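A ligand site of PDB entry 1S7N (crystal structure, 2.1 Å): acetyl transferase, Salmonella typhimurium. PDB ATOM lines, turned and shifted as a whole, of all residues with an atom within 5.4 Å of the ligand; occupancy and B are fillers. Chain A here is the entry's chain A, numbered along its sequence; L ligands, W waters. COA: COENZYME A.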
ATOM      1  N   TRP A  37      34.733   0.513  17.292  1.00  0.00           N
ATOM      2  CA  TRP A  37      33.634   0.448  18.256  1.00  0.00           C
ATOM      3  C   TRP A  37      33.752  -0.796  19.094  1.00  0.00           C
ATOM      4  O   TRP A  37      33.775  -0.711  20.304  1.00  0.00           O
ATOM      5  CB  TRP A  37      32.292   0.481  17.533  1.00  0.00           C
ATOM      6  CG  TRP A  37      31.113  -0.195  18.215  1.00  0.00           C
ATOM      7  CD1 TRP A  37      30.321  -1.222  17.706  1.00  0.00           C
ATOM      8  CD2 TRP A  37      30.480   0.218  19.419  1.00  0.00           C
ATOM      9  NE1 TRP A  37      29.209  -1.445  18.526  1.00  0.00           N
ATOM     10  CE2 TRP A  37      29.286  -0.566  19.581  1.00  0.00           C
ATOM     11  CE3 TRP A  37      30.792   1.190  20.379  1.00  0.00           C
ATOM     12  CZ2 TRP A  37      28.434  -0.411  20.656  1.00  0.00           C
ATOM     13  CZ3 TRP A  37      29.903   1.341  21.481  1.00  0.00           C
ATOM     14  CH2 TRP A  37      28.762   0.563  21.603  1.00  0.00           C
ATOM     15  N   LEU A  38      33.820  -1.961  18.463  1.00  0.00           N
ATOM     16  CA  LEU A  38      33.878  -3.204  19.238  1.00  0.00           C
ATOM     17  C   LEU A  38      35.063  -3.367  20.213  1.00  0.00           C
ATOM     18  O   LEU A  38      34.960  -4.032  21.255  1.00  0.00           O
ATOM     19  CB  LEU A  38      33.859  -4.355  18.284  1.00  0.00           C
ATOM     20  CG  LEU A  38      32.588  -4.546  17.438  1.00  0.00           C
ATOM     21  CD1 LEU A  38      32.904  -5.710  16.457  1.00  0.00           C
ATOM     22  CD2 LEU A  38      31.346  -4.797  18.313  1.00  0.00           C
ATOM     23  N   SER A  41      34.889  -2.824  23.855  1.00  0.00           N
ATOM     24  CA  SER A  41      34.292  -3.774  24.776  1.00  0.00           C
ATOM     25  C   SER A  41      34.762  -5.168  24.628  1.00  0.00           C
ATOM     26  O   SER A  41      34.485  -5.983  25.492  1.00  0.00           O
ATOM     27  CB  SER A  41      32.755  -3.833  24.574  1.00  0.00           C
ATOM     28  OG  SER A  41      32.153  -2.546  24.651  1.00  0.00           O
ATOM     29  N   LEU A  42      35.443  -5.425  23.518  1.00  0.00           N
ATOM     30  CA  LEU A  42      35.863  -6.767  23.183  1.00  0.00           C
ATOM     31  C   LEU A  42      37.321  -6.836  22.807  1.00  0.00           C
ATOM     32  O   LEU A  42      37.835  -5.920  22.167  1.00  0.00           O
ATOM     33  CB  LEU A  42      35.050  -7.210  21.962  1.00  0.00           C
ATOM     34  CG  LEU A  42      33.553  -7.249  22.257  1.00  0.00           C
ATOM     35  CD1 LEU A  42      32.741  -7.350  20.988  1.00  0.00           C
ATOM     36  CD2 LEU A  42      33.269  -8.444  23.150  1.00  0.00           C
ATOM     37  N   TYR A 101      27.153 -11.346  22.419  1.00  0.00           N
ATOM     38  CA  TYR A 101      26.472 -10.543  21.434  1.00  0.00           C
ATOM     39  C   TYR A 101      27.170  -9.216  21.164  1.00  0.00           C
ATOM     40  O   TYR A 101      28.003  -8.750  21.934  1.00  0.00           O
ATOM     41  CB  TYR A 101      25.009 -10.237  21.844  1.00  0.00           C
ATOM     42  CG  TYR A 101      24.830  -9.874  23.300  1.00  0.00           C
ATOM     43  CD1 TYR A 101      25.316  -8.679  23.806  1.00  0.00           C
ATOM     44  CD2 TYR A 101      24.176 -10.737  24.194  1.00  0.00           C
ATOM     45  CE1 TYR A 101      25.171  -8.328  25.142  1.00  0.00           C
ATOM     46  CE2 TYR A 101      24.022 -10.392  25.570  1.00  0.00           C
ATOM     47  CZ  TYR A 101      24.522  -9.200  26.026  1.00  0.00           C
ATOM     48  OH  TYR A 101      24.421  -8.862  27.383  1.00  0.00           O
ATOM     49  N   TRP A 102      26.753  -8.620  20.053  1.00  0.00           N
ATOM     50  CA  TRP A 102      27.203  -7.312  19.622  1.00  0.00           C
ATOM     51  C   TRP A 102      26.318  -6.854  18.482  1.00  0.00           C
ATOM     52  O   TRP A 102      25.721  -7.650  17.778  1.00  0.00           O
ATOM     53  CB  TRP A 102      28.708  -7.275  19.218  1.00  0.00           C
ATOM     54  CG  TRP A 102      29.128  -8.055  17.988  1.00  0.00           C
ATOM     55  CD1 TRP A 102      29.708  -9.305  17.939  1.00  0.00           C
ATOM     56  CD2 TRP A 102      29.163  -7.574  16.657  1.00  0.00           C
ATOM     57  NE1 TRP A 102      30.110  -9.610  16.659  1.00  0.00           N
ATOM     58  CE2 TRP A 102      29.770  -8.549  15.851  1.00  0.00           C
ATOM     59  CE3 TRP A 102      28.733  -6.384  16.061  1.00  0.00           C
ATOM     60  CZ2 TRP A 102      29.965  -8.381  14.496  1.00  0.00           C
ATOM     61  CZ3 TRP A 102      28.933  -6.209  14.720  1.00  0.00           C
ATOM     62  CH2 TRP A 102      29.553  -7.210  13.951  1.00  0.00           C
ATOM     63  N   LEU A 103      26.198  -5.547  18.374  1.00  0.00           N
ATOM     64  CA  LEU A 103      25.402  -4.887  17.344  1.00  0.00           C
ATOM     65  C   LEU A 103      26.244  -3.847  16.650  1.00  0.00           C
ATOM     66  O   LEU A 103      27.114  -3.224  17.260  1.00  0.00           O
ATOM     67  CB  LEU A 103      24.263  -4.095  17.968  1.00  0.00           C
ATOM     68  CG  LEU A 103      23.000  -4.813  18.422  1.00  0.00           C
ATOM     69  CD1 LEU A 103      22.057  -3.739  18.905  1.00  0.00           C
ATOM     70  CD2 LEU A 103      22.393  -5.536  17.273  1.00  0.00           C
ATOM     71  N   PHE A 107      22.803   0.509  15.338  1.00  0.00           N
ATOM     72  CA  PHE A 107      21.513  -0.164  15.582  1.00  0.00           C
ATOM     73  C   PHE A 107      21.151  -0.268  17.067  1.00  0.00           C
ATOM     74  O   PHE A 107      20.205  -0.994  17.464  1.00  0.00           O
ATOM     75  CB  PHE A 107      21.505  -1.560  14.946  1.00  0.00           C
ATOM     76  CG  PHE A 107      21.329  -1.564  13.446  1.00  0.00           C
ATOM     77  CD1 PHE A 107      22.433  -1.549  12.601  1.00  0.00           C
ATOM     78  CD2 PHE A 107      20.052  -1.699  12.876  1.00  0.00           C
ATOM     79  CE1 PHE A 107      22.272  -1.682  11.202  1.00  0.00           C
ATOM     80  CE2 PHE A 107      19.870  -1.828  11.455  1.00  0.00           C
ATOM     81  CZ  PHE A 107      20.964  -1.825  10.626  1.00  0.00           C
ATOM     82  N   GLN A 108      21.913   0.452  17.897  1.00  0.00           N
ATOM     83  CA  GLN A 108      21.686   0.475  19.334  1.00  0.00           C
ATOM     84  C   GLN A 108      20.461   1.327  19.665  1.00  0.00           C
ATOM     85  O   GLN A 108      20.037   2.168  18.848  1.00  0.00           O
ATOM     86  CB  GLN A 108      22.883   1.071  20.070  1.00  0.00           C
ATOM     87  CG  GLN A 108      24.079   0.163  20.089  1.00  0.00           C
ATOM     88  CD  GLN A 108      25.224   0.871  20.703  1.00  0.00           C
ATOM     89  OE1 GLN A 108      25.594   0.606  21.841  1.00  0.00           O
ATOM     90  NE2 GLN A 108      25.782   1.843  19.958  1.00  0.00           N
ATOM     91  N   GLY A 109      19.906   1.122  20.857  1.00  0.00           N
ATOM     92  CA  GLY A 109      18.756   1.898  21.270  1.00  0.00           C
ATOM     93  C   GLY A 109      17.399   1.525  20.679  1.00  0.00           C
ATOM     94  O   GLY A 109      16.479   2.316  20.781  1.00  0.00           O
ATOM     95  N   GLN A 110      17.225   0.358  20.086  1.00  0.00           N
ATOM     96  CA  GLN A 110      15.891   0.017  19.546  1.00  0.00           C
ATOM     97  C   GLN A 110      15.450  -1.323  20.044  1.00  0.00           C
ATOM     98  O   GLN A 110      14.589  -1.937  19.440  1.00  0.00           O
ATOM     99  CB  GLN A 110      15.937  -0.041  18.036  1.00  0.00           C
ATOM    100  CG  GLN A 110      16.528   1.178  17.391  1.00  0.00           C
ATOM    101  CD  GLN A 110      16.776   0.893  15.947  1.00  0.00           C
ATOM    102  OE1 GLN A 110      15.899   0.403  15.263  1.00  0.00           O
ATOM    103  NE2 GLN A 110      17.977   1.181  15.464  1.00  0.00           N
ATOM    104  N   GLY A 111      16.070  -1.806  21.127  1.00  0.00           N
ATOM    105  CA  GLY A 111      15.692  -3.119  21.639  1.00  0.00           C
ATOM    106  C   GLY A 111      15.959  -4.293  20.666  1.00  0.00           C
ATOM    107  O   GLY A 111      15.407  -5.415  20.838  1.00  0.00           O
ATOM    108  N   ILE A 112      16.760  -4.079  19.633  1.00  0.00           N
ATOM    109  CA  ILE A 112      17.042  -5.170  18.714  1.00  0.00           C
ATOM    110  C   ILE A 112      17.701  -6.379  19.456  1.00  0.00           C
ATOM    111  O   ILE A 112      17.320  -7.520  19.226  1.00  0.00           O
ATOM    112  CB  ILE A 112      17.911  -4.673  17.555  1.00  0.00           C
ATOM    113  CG1 ILE A 112      17.071  -3.781  16.662  1.00  0.00           C
ATOM    114  CG2 ILE A 112      18.459  -5.895  16.659  1.00  0.00           C
ATOM    115  CD1 ILE A 112      17.956  -2.949  15.744  1.00  0.00           C
ATOM    116  N   MET A 113      18.655  -6.128  20.345  1.00  0.00           N
ATOM    117  CA  MET A 113      19.293  -7.233  21.014  1.00  0.00           C
ATOM    118  C   MET A 113      18.317  -7.881  21.995  1.00  0.00           C
ATOM    119  O   MET A 113      18.169  -9.116  22.002  1.00  0.00           O
ATOM    120  CB  MET A 113      20.559  -6.805  21.781  1.00  0.00           C
ATOM    121  CG  MET A 113      21.421  -8.039  22.282  1.00  0.00           C
ATOM    122  SD  MET A 113      21.805  -9.253  20.922  1.00  0.00           S
ATOM    123  CE  MET A 113      22.833  -8.146  19.857  1.00  0.00           C
ATOM    124  N   SER A 114      17.636  -7.091  22.825  1.00  0.00           N
ATOM    125  CA  SER A 114      16.683  -7.673  23.771  1.00  0.00           C
ATOM    126  C   SER A 114      15.616  -8.539  23.058  1.00  0.00           C
ATOM    127  O   SER A 114      15.342  -9.707  23.475  1.00  0.00           O
ATOM    128  CB  SER A 114      15.981  -6.568  24.594  1.00  0.00           C
ATOM    129  OG  SER A 114      16.820  -6.075  25.632  1.00  0.00           O
ATOM    130  N   GLN A 115      15.032  -7.997  21.980  1.00  0.00           N
ATOM    131  CA  GLN A 115      14.028  -8.782  21.267  1.00  0.00           C
ATOM    132  C   GLN A 115      14.627 -10.075  20.735  1.00  0.00           C
ATOM    133  O   GLN A 115      14.036 -11.139  20.863  1.00  0.00           O
ATOM    134  CB  GLN A 115      13.435  -8.008  20.073  1.00  0.00           C
ATOM    135  CG  GLN A 115      12.677  -6.769  20.460  1.00  0.00           C
ATOM    136  CD  GLN A 115      12.154  -6.060  19.223  1.00  0.00           C
ATOM    137  OE1 GLN A 115      11.223  -6.535  18.583  1.00  0.00           O
ATOM    138  NE2 GLN A 115      12.784  -4.949  18.863  1.00  0.00           N
ATOM    139  N   ILE A 135      25.117 -14.999  31.043  1.00  0.00           N
ATOM    140  CA  ILE A 135      25.756 -13.833  30.469  1.00  0.00           C
ATOM    141  C   ILE A 135      26.907 -13.356  31.322  1.00  0.00           C
ATOM    142  O   ILE A 135      26.761 -13.019  32.497  1.00  0.00           O
ATOM    143  CB  ILE A 135      24.784 -12.657  30.276  1.00  0.00           C
ATOM    144  CG1 ILE A 135      23.898 -12.913  29.037  1.00  0.00           C
ATOM    145  CG2 ILE A 135      25.593 -11.374  30.021  1.00  0.00           C
ATOM    146  CD1 ILE A 135      22.704 -11.859  28.929  1.00  0.00           C
ATOM    147  N   LYS A 136      28.092 -13.412  30.778  1.00  0.00           N
ATOM    148  CA  LYS A 136      29.221 -12.888  31.525  1.00  0.00           C
ATOM    149  C   LYS A 136      29.519 -11.524  30.959  1.00  0.00           C
ATOM    150  O   LYS A 136      29.612 -11.347  29.746  1.00  0.00           O
ATOM    151  CB  LYS A 136      30.442 -13.792  31.331  1.00  0.00           C
ATOM    152  CG  LYS A 136      30.607 -14.739  32.453  1.00  0.00           C
ATOM    153  CD  LYS A 136      31.120 -16.066  31.953  1.00  0.00           C
ATOM    154  CE  LYS A 136      32.547 -15.899  31.508  1.00  0.00           C
ATOM    155  NZ  LYS A 136      33.025 -17.060  30.677  1.00  0.00           N
ATOM    156  N   CYS A 137      29.616 -10.521  31.816  1.00  0.00           N
ATOM    157  CA  CYS A 137      29.945  -9.215  31.290  1.00  0.00           C
ATOM    158  C   CYS A 137      30.586  -8.287  32.296  1.00  0.00           C
ATOM    159  O   CYS A 137      30.197  -8.259  33.471  1.00  0.00           O
ATOM    160  CB  CYS A 137      28.741  -8.532  30.668  1.00  0.00           C
ATOM    161  SG  CYS A 137      27.516  -7.952  31.792  1.00  0.00           S
ATOM    162  N   ARG A 138      31.562  -7.555  31.791  1.00  0.00           N
ATOM    163  CA  ARG A 138      32.314  -6.626  32.592  1.00  0.00           C
ATOM    164  C   ARG A 138      31.438  -5.750  33.474  1.00  0.00           C
ATOM    165  O   ARG A 138      30.378  -5.303  33.035  1.00  0.00           O
ATOM    166  CB  ARG A 138      33.178  -5.774  31.677  1.00  0.00           C
ATOM    167  CG  ARG A 138      34.373  -6.521  31.269  1.00  0.00           C
ATOM    168  CD  ARG A 138      35.292  -5.656  30.518  1.00  0.00           C
ATOM    169  NE  ARG A 138      34.657  -5.181  29.303  1.00  0.00           N
ATOM    170  CZ  ARG A 138      34.267  -3.931  29.142  1.00  0.00           C
ATOM    171  NH1 ARG A 138      34.456  -3.049  30.106  1.00  0.00           N
ATOM    172  NH2 ARG A 138      33.697  -3.561  27.999  1.00  0.00           N
ATOM    173  N   ASN A 141      30.639  -2.524  31.753  1.00  0.00           N
ATOM    174  CA  ASN A 141      30.072  -2.455  30.407  1.00  0.00           C
ATOM    175  C   ASN A 141      28.581  -2.147  30.690  1.00  0.00           C
ATOM    176  O   ASN A 141      27.787  -3.097  30.891  1.00  0.00           O
ATOM    177  CB  ASN A 141      30.216  -3.801  29.697  1.00  0.00           C
ATOM    178  CG  ASN A 141      29.706  -3.757  28.251  1.00  0.00           C
ATOM    179  OD1 ASN A 141      28.774  -2.984  27.915  1.00  0.00           O
ATOM    180  ND2 ASN A 141      30.292  -4.611  27.397  1.00  0.00           N
ATOM    181  N   ALA A 143      26.058  -0.921  28.826  1.00  0.00           N
ATOM    182  CA  ALA A 143      25.130  -1.413  27.857  1.00  0.00           C
ATOM    183  C   ALA A 143      24.840  -2.930  28.054  1.00  0.00           C
ATOM    184  O   ALA A 143      23.664  -3.357  28.020  1.00  0.00           O
ATOM    185  CB  ALA A 143      25.693  -1.147  26.475  1.00  0.00           C
ATOM    186  N   SER A 144      25.895  -3.735  28.266  1.00  0.00           N
ATOM    187  CA  SER A 144      25.668  -5.171  28.395  1.00  0.00           C
ATOM    188  C   SER A 144      24.943  -5.486  29.665  1.00  0.00           C
ATOM    189  O   SER A 144      24.007  -6.264  29.641  1.00  0.00           O
ATOM    190  CB  SER A 144      26.964  -5.968  28.345  1.00  0.00           C
ATOM    191  OG  SER A 144      26.655  -7.345  28.125  1.00  0.00           O
ATOM    192  N   VAL A 147      21.464  -4.987  29.140  1.00  0.00           N
ATOM    193  CA  VAL A 147      20.808  -6.064  28.431  1.00  0.00           C
ATOM    194  C   VAL A 147      20.454  -7.201  29.411  1.00  0.00           C
ATOM    195  O   VAL A 147      19.335  -7.725  29.403  1.00  0.00           O
ATOM    196  CB  VAL A 147      21.702  -6.623  27.280  1.00  0.00           C
ATOM    197  CG1 VAL A 147      21.106  -7.946  26.767  1.00  0.00           C
ATOM    198  CG2 VAL A 147      21.729  -5.652  26.111  1.00  0.00           C
ATOM    199  N   ARG A 150      17.485  -5.925  31.880  1.00  0.00           N
ATOM    200  CA  ARG A 150      16.280  -5.726  31.116  1.00  0.00           C
ATOM    201  C   ARG A 150      15.626  -7.078  30.784  1.00  0.00           C
ATOM    202  O   ARG A 150      14.376  -7.238  30.799  1.00  0.00           O
ATOM    203  CB  ARG A 150      16.612  -4.935  29.835  1.00  0.00           C
ATOM    204  CG  ARG A 150      15.378  -4.592  28.999  1.00  0.00           C
ATOM    205  CD  ARG A 150      15.671  -3.729  27.720  1.00  0.00           C
ATOM    206  NE  ARG A 150      16.662  -2.656  27.919  1.00  0.00           N
ATOM    207  CZ  ARG A 150      16.416  -1.420  28.381  1.00  0.00           C
ATOM    208  NH1 ARG A 150      15.164  -1.034  28.717  1.00  0.00           N
ATOM    209  NH2 ARG A 150      17.443  -0.582  28.528  1.00  0.00           N
ATOM    210  N   ASN A 151      16.461  -8.091  30.560  1.00  0.00           N
ATOM    211  CA  ASN A 151      15.920  -9.382  30.215  1.00  0.00           C
ATOM    212  C   ASN A 151      15.730 -10.400  31.318  1.00  0.00           C
ATOM    213  O   ASN A 151      15.679 -11.627  31.081  1.00  0.00           O
ATOM    214  CB  ASN A 151      16.716  -9.915  29.041  1.00  0.00           C
ATOM    215  CG  ASN A 151      16.503  -9.081  27.810  1.00  0.00           C
ATOM    216  OD1 ASN A 151      15.519  -9.271  27.108  1.00  0.00           O
ATOM    217  ND2 ASN A 151      17.400  -8.125  27.560  1.00  0.00           N
HETATM  218  N1A COA L   1      12.421  -3.228  23.688  1.00  0.00           N
HETATM  219  C2A COA L   1      13.500  -3.040  24.516  1.00  0.00           C
HETATM  220  N3A COA L   1      14.290  -1.948  24.560  1.00  0.00           N
HETATM  221  C4A COA L   1      13.962  -0.925  23.673  1.00  0.00           C
HETATM  222  C5A COA L   1      12.885  -1.033  22.790  1.00  0.00           C
HETATM  223  C6A COA L   1      12.094  -2.215  22.799  1.00  0.00           C
HETATM  224  N6A COA L   1      11.049  -2.271  21.906  1.00  0.00           N
HETATM  225  N7A COA L   1      12.734   0.083  21.995  1.00  0.00           N
HETATM  226  C8A COA L   1      13.691   0.898  22.351  1.00  0.00           C
HETATM  227  N9A COA L   1      14.439   0.317  23.335  1.00  0.00           N
HETATM  228  C1B COA L   1      15.586   0.931  23.903  1.00  0.00           C
HETATM  229  C2B COA L   1      15.733   0.793  25.411  1.00  0.00           C
HETATM  230  O2B COA L   1      15.010   1.880  26.041  1.00  0.00           O
HETATM  231  C3B COA L   1      17.231   0.986  25.536  1.00  0.00           C
HETATM  232  O3B COA L   1      17.572   2.343  25.317  1.00  0.00           O
HETATM  233  P3B COA L   1      18.719   3.017  26.266  1.00  0.00           P
HETATM  234  O7A COA L   1      18.609   4.464  25.982  1.00  0.00           O
HETATM  235  O8A COA L   1      20.051   2.385  25.944  1.00  0.00           O
HETATM  236  O9A COA L   1      18.268   2.745  27.669  1.00  0.00           O
HETATM  237  C4B COA L   1      17.717   0.102  24.379  1.00  0.00           C
HETATM  238  O4B COA L   1      16.775   0.365  23.315  1.00  0.00           O
HETATM  239  C5B COA L   1      17.829  -1.403  24.644  1.00  0.00           C
HETATM  240  O5B COA L   1      18.148  -2.073  23.436  1.00  0.00           O
HETATM  241  P1A COA L   1      18.851  -3.531  23.530  1.00  0.00           P
HETATM  242  O1A COA L   1      18.580  -4.175  24.830  1.00  0.00           O
HETATM  243  O2A COA L   1      18.404  -4.267  22.323  1.00  0.00           O
HETATM  244  O3A COA L   1      20.385  -3.285  23.455  1.00  0.00           O
HETATM  245  P2A COA L   1      21.259  -2.044  23.011  1.00  0.00           P
HETATM  246  O4A COA L   1      20.778  -1.438  21.780  1.00  0.00           O
HETATM  247  O5A COA L   1      21.453  -1.156  24.125  1.00  0.00           O
HETATM  248  O6A COA L   1      22.728  -2.614  22.789  1.00  0.00           O
HETATM  249  CBP COA L   1      24.629  -3.995  23.257  1.00  0.00           C
HETATM  250  CCP COA L   1      23.384  -3.343  23.818  1.00  0.00           C
HETATM  251  CDP COA L   1      25.495  -4.564  24.461  1.00  0.00           C
HETATM  252  CEP COA L   1      24.215  -5.219  22.365  1.00  0.00           C
HETATM  253  CAP COA L   1      25.451  -2.971  22.416  1.00  0.00           C
HETATM  254  OAP COA L   1      25.746  -1.868  23.252  1.00  0.00           O
HETATM  255  C9P COA L   1      26.774  -3.520  21.831  1.00  0.00           C
HETATM  256  O9P COA L   1      26.822  -4.168  20.773  1.00  0.00           O
HETATM  257  N8P COA L   1      27.873  -3.205  22.621  1.00  0.00           N
HETATM  258  C7P COA L   1      29.257  -3.431  22.229  1.00  0.00           C
HETATM  259  C6P COA L   1      29.655  -4.930  22.299  1.00  0.00           C
HETATM  260  C5P COA L   1      29.448  -5.521  23.708  1.00  0.00           C
HETATM  261  O5P COA L   1      29.437  -4.812  24.703  1.00  0.00           O
HETATM  262  N4P COA L   1      28.928  -6.839  23.707  1.00  0.00           N
HETATM  263  C3P COA L   1      28.574  -7.575  24.907  1.00  0.00           C
HETATM  264  C2P COA L   1      29.767  -8.157  25.595  1.00  0.00           C
HETATM  265  S1P COA L   1      29.268  -8.898  27.207  1.00  0.00           S
HETATM  266  O   HOH W   1      31.805  -1.310  22.217  1.00  0.00           O
HETATM  267  O   HOH W   2      21.205   0.697  27.820  1.00  0.00           O
HETATM  268  O   HOH W   3      29.828 -10.368  23.615  1.00  0.00           O
HETATM  269  O   HOH W   4      12.990  -2.334  27.688  1.00  0.00           O
HETATM  270  O   HOH W   5      19.259  -3.080  27.472  1.00  0.00           O
HETATM  271  O   HOH W   6      31.956  -7.307  28.685  1.00  0.00           O
HETATM  272  O   HOH W   7      21.566  -1.899  26.731  1.00  0.00           O
HETATM  273  O   HOH W   8      29.102  -2.164  25.406  1.00  0.00           O
HETATM  274  O   HOH W   9      18.888  -1.870  19.447  1.00  0.00           O
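Water W7 bridges O5A of the ligand (2.7 Å) and O of Ala 143 (2.9 Å).
Water W8 lies within hydrogen-bond range of OD1 of Asn 141 (2.7 Å), O5P of the ligand (2.8 Å) and OG of Ser 41 (3.2 Å).
Water W5 lies within hydrogen-bond range of NE of Arg 150, O1A of the ligand and N of Val 147.
Water W4 lies within hydrogen-bond range of the guanidinium group of Arg 150 (2.7 Å) and a nitrogen (N3A) of the ligand (3.4 Å).
Water W1 bridges OG of Ser 41 (2.8 Å) and O of Trp 37 (2.8 Å).
Water W6 lies within hydrogen-bond range of N of Arg 138 (3.1 Å), ND2 of Asn 141 (3.4 Å) and S1P of the ligand (3.5 Å).
Merely in contact with the ligand: Trp 37 (3.5 Å), Ser 41 (3.5 Å), Trp 102 (3.4 Å), Cys 137 (3.5 Å), Ala 143 (3.3 Å) and Val 147 (3.7 Å).
Hydrophobic or aromatic side chains within 4 Å of the ligand: Trp 37, Tyr 101, Trp 102, Leu 103, Met 113, Ala 143 and Val 147.
19 residues have an atom within 4 Å of the ligand: Trp 37, Ser 41, Tyr 101, Trp 102, Leu 103, Gln 108, Gly 109, Gln 110, Gly 111, Ile 112, Met 113, Ser 114, Lys 136, Cys 137, Asn 141, Ala 143, Ser 144, Val 147 and Arg 150.
The side-chain amide nitrogen (ND2) of Asn 151 is in hydrogen-bond range of the side-chain hydroxyl (OG) of Ser 114 (2.9 Å).
NE2 of Gln 115 sits close to O of Gly 111 (3.3 Å).
O of Val 147 sits at hydrogen-bond distance from ND2 of Asn 151, 2.7 Å away.
OG of Ser 144 sits at hydrogen-bond distance from OH of Tyr 101, at 2.8 Å.
The backbone NH (N) of Ser 144 sits at hydrogen-bond distance from the side-chain amide oxygen (OD1) of Asn 141 (3.0 Å).
The backbone carbonyl oxygen (O) of Leu 103 is in hydrogen-bond range of the indole nitrogen (NE1) of Trp 37.
OE1 of Gln 108 lies within hydrogen-bond range of OAP of the ligand (2.9 Å).
The backbone NH (N) of Ser 114 is in hydrogen-bond range of an oxygen (O2A) of the ligand (3.0 Å).
ND2 of Asn 141 is in hydrogen-bond range of O5P of the ligand (2.8 Å).
The guanidinium group of Arg 150 is in salt-bridge range of an oxygen (O9A) of the ligand (3.5 Å).
O9P of the ligand sits at hydrogen-bond distance from N of Leu 103.
OG of Ser 144 lies close to S1P of the ligand, at 3.2 Å.
The backbone NH (N) of Met 113 lies within hydrogen-bond range of an oxygen (O2A) of the ligand, 2.7 Å away.
The backbone NH (N) of Gln 110 is in hydrogen-bond range of an oxygen (O4B) of the ligand (3.3 Å).
An oxygen (O4A) of the ligand is in hydrogen-bond range of the backbone NH (N) of Gly 109.
An oxygen (O1A) of the ligand is in hydrogen-bond range of the side-chain hydroxyl (OG) of Ser 114, at 2.7 Å.
The backbone NH (N) of Gly 111 sits at hydrogen-bond distance from an oxygen (O5B) of the ligand (3.1 Å).
The backbone carbonyl oxygen (O) of Tyr 101 lies within hydrogen-bond range of a nitrogen (N4P) of the ligand, at 2.8 Å.
The backbone NH (N) of Ile 112 lies within hydrogen-bond range of an oxygen (O2A) of the ligand (3.2 Å).
O of Lys 136 sits close to S1P of the ligand, 3.5 Å away.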
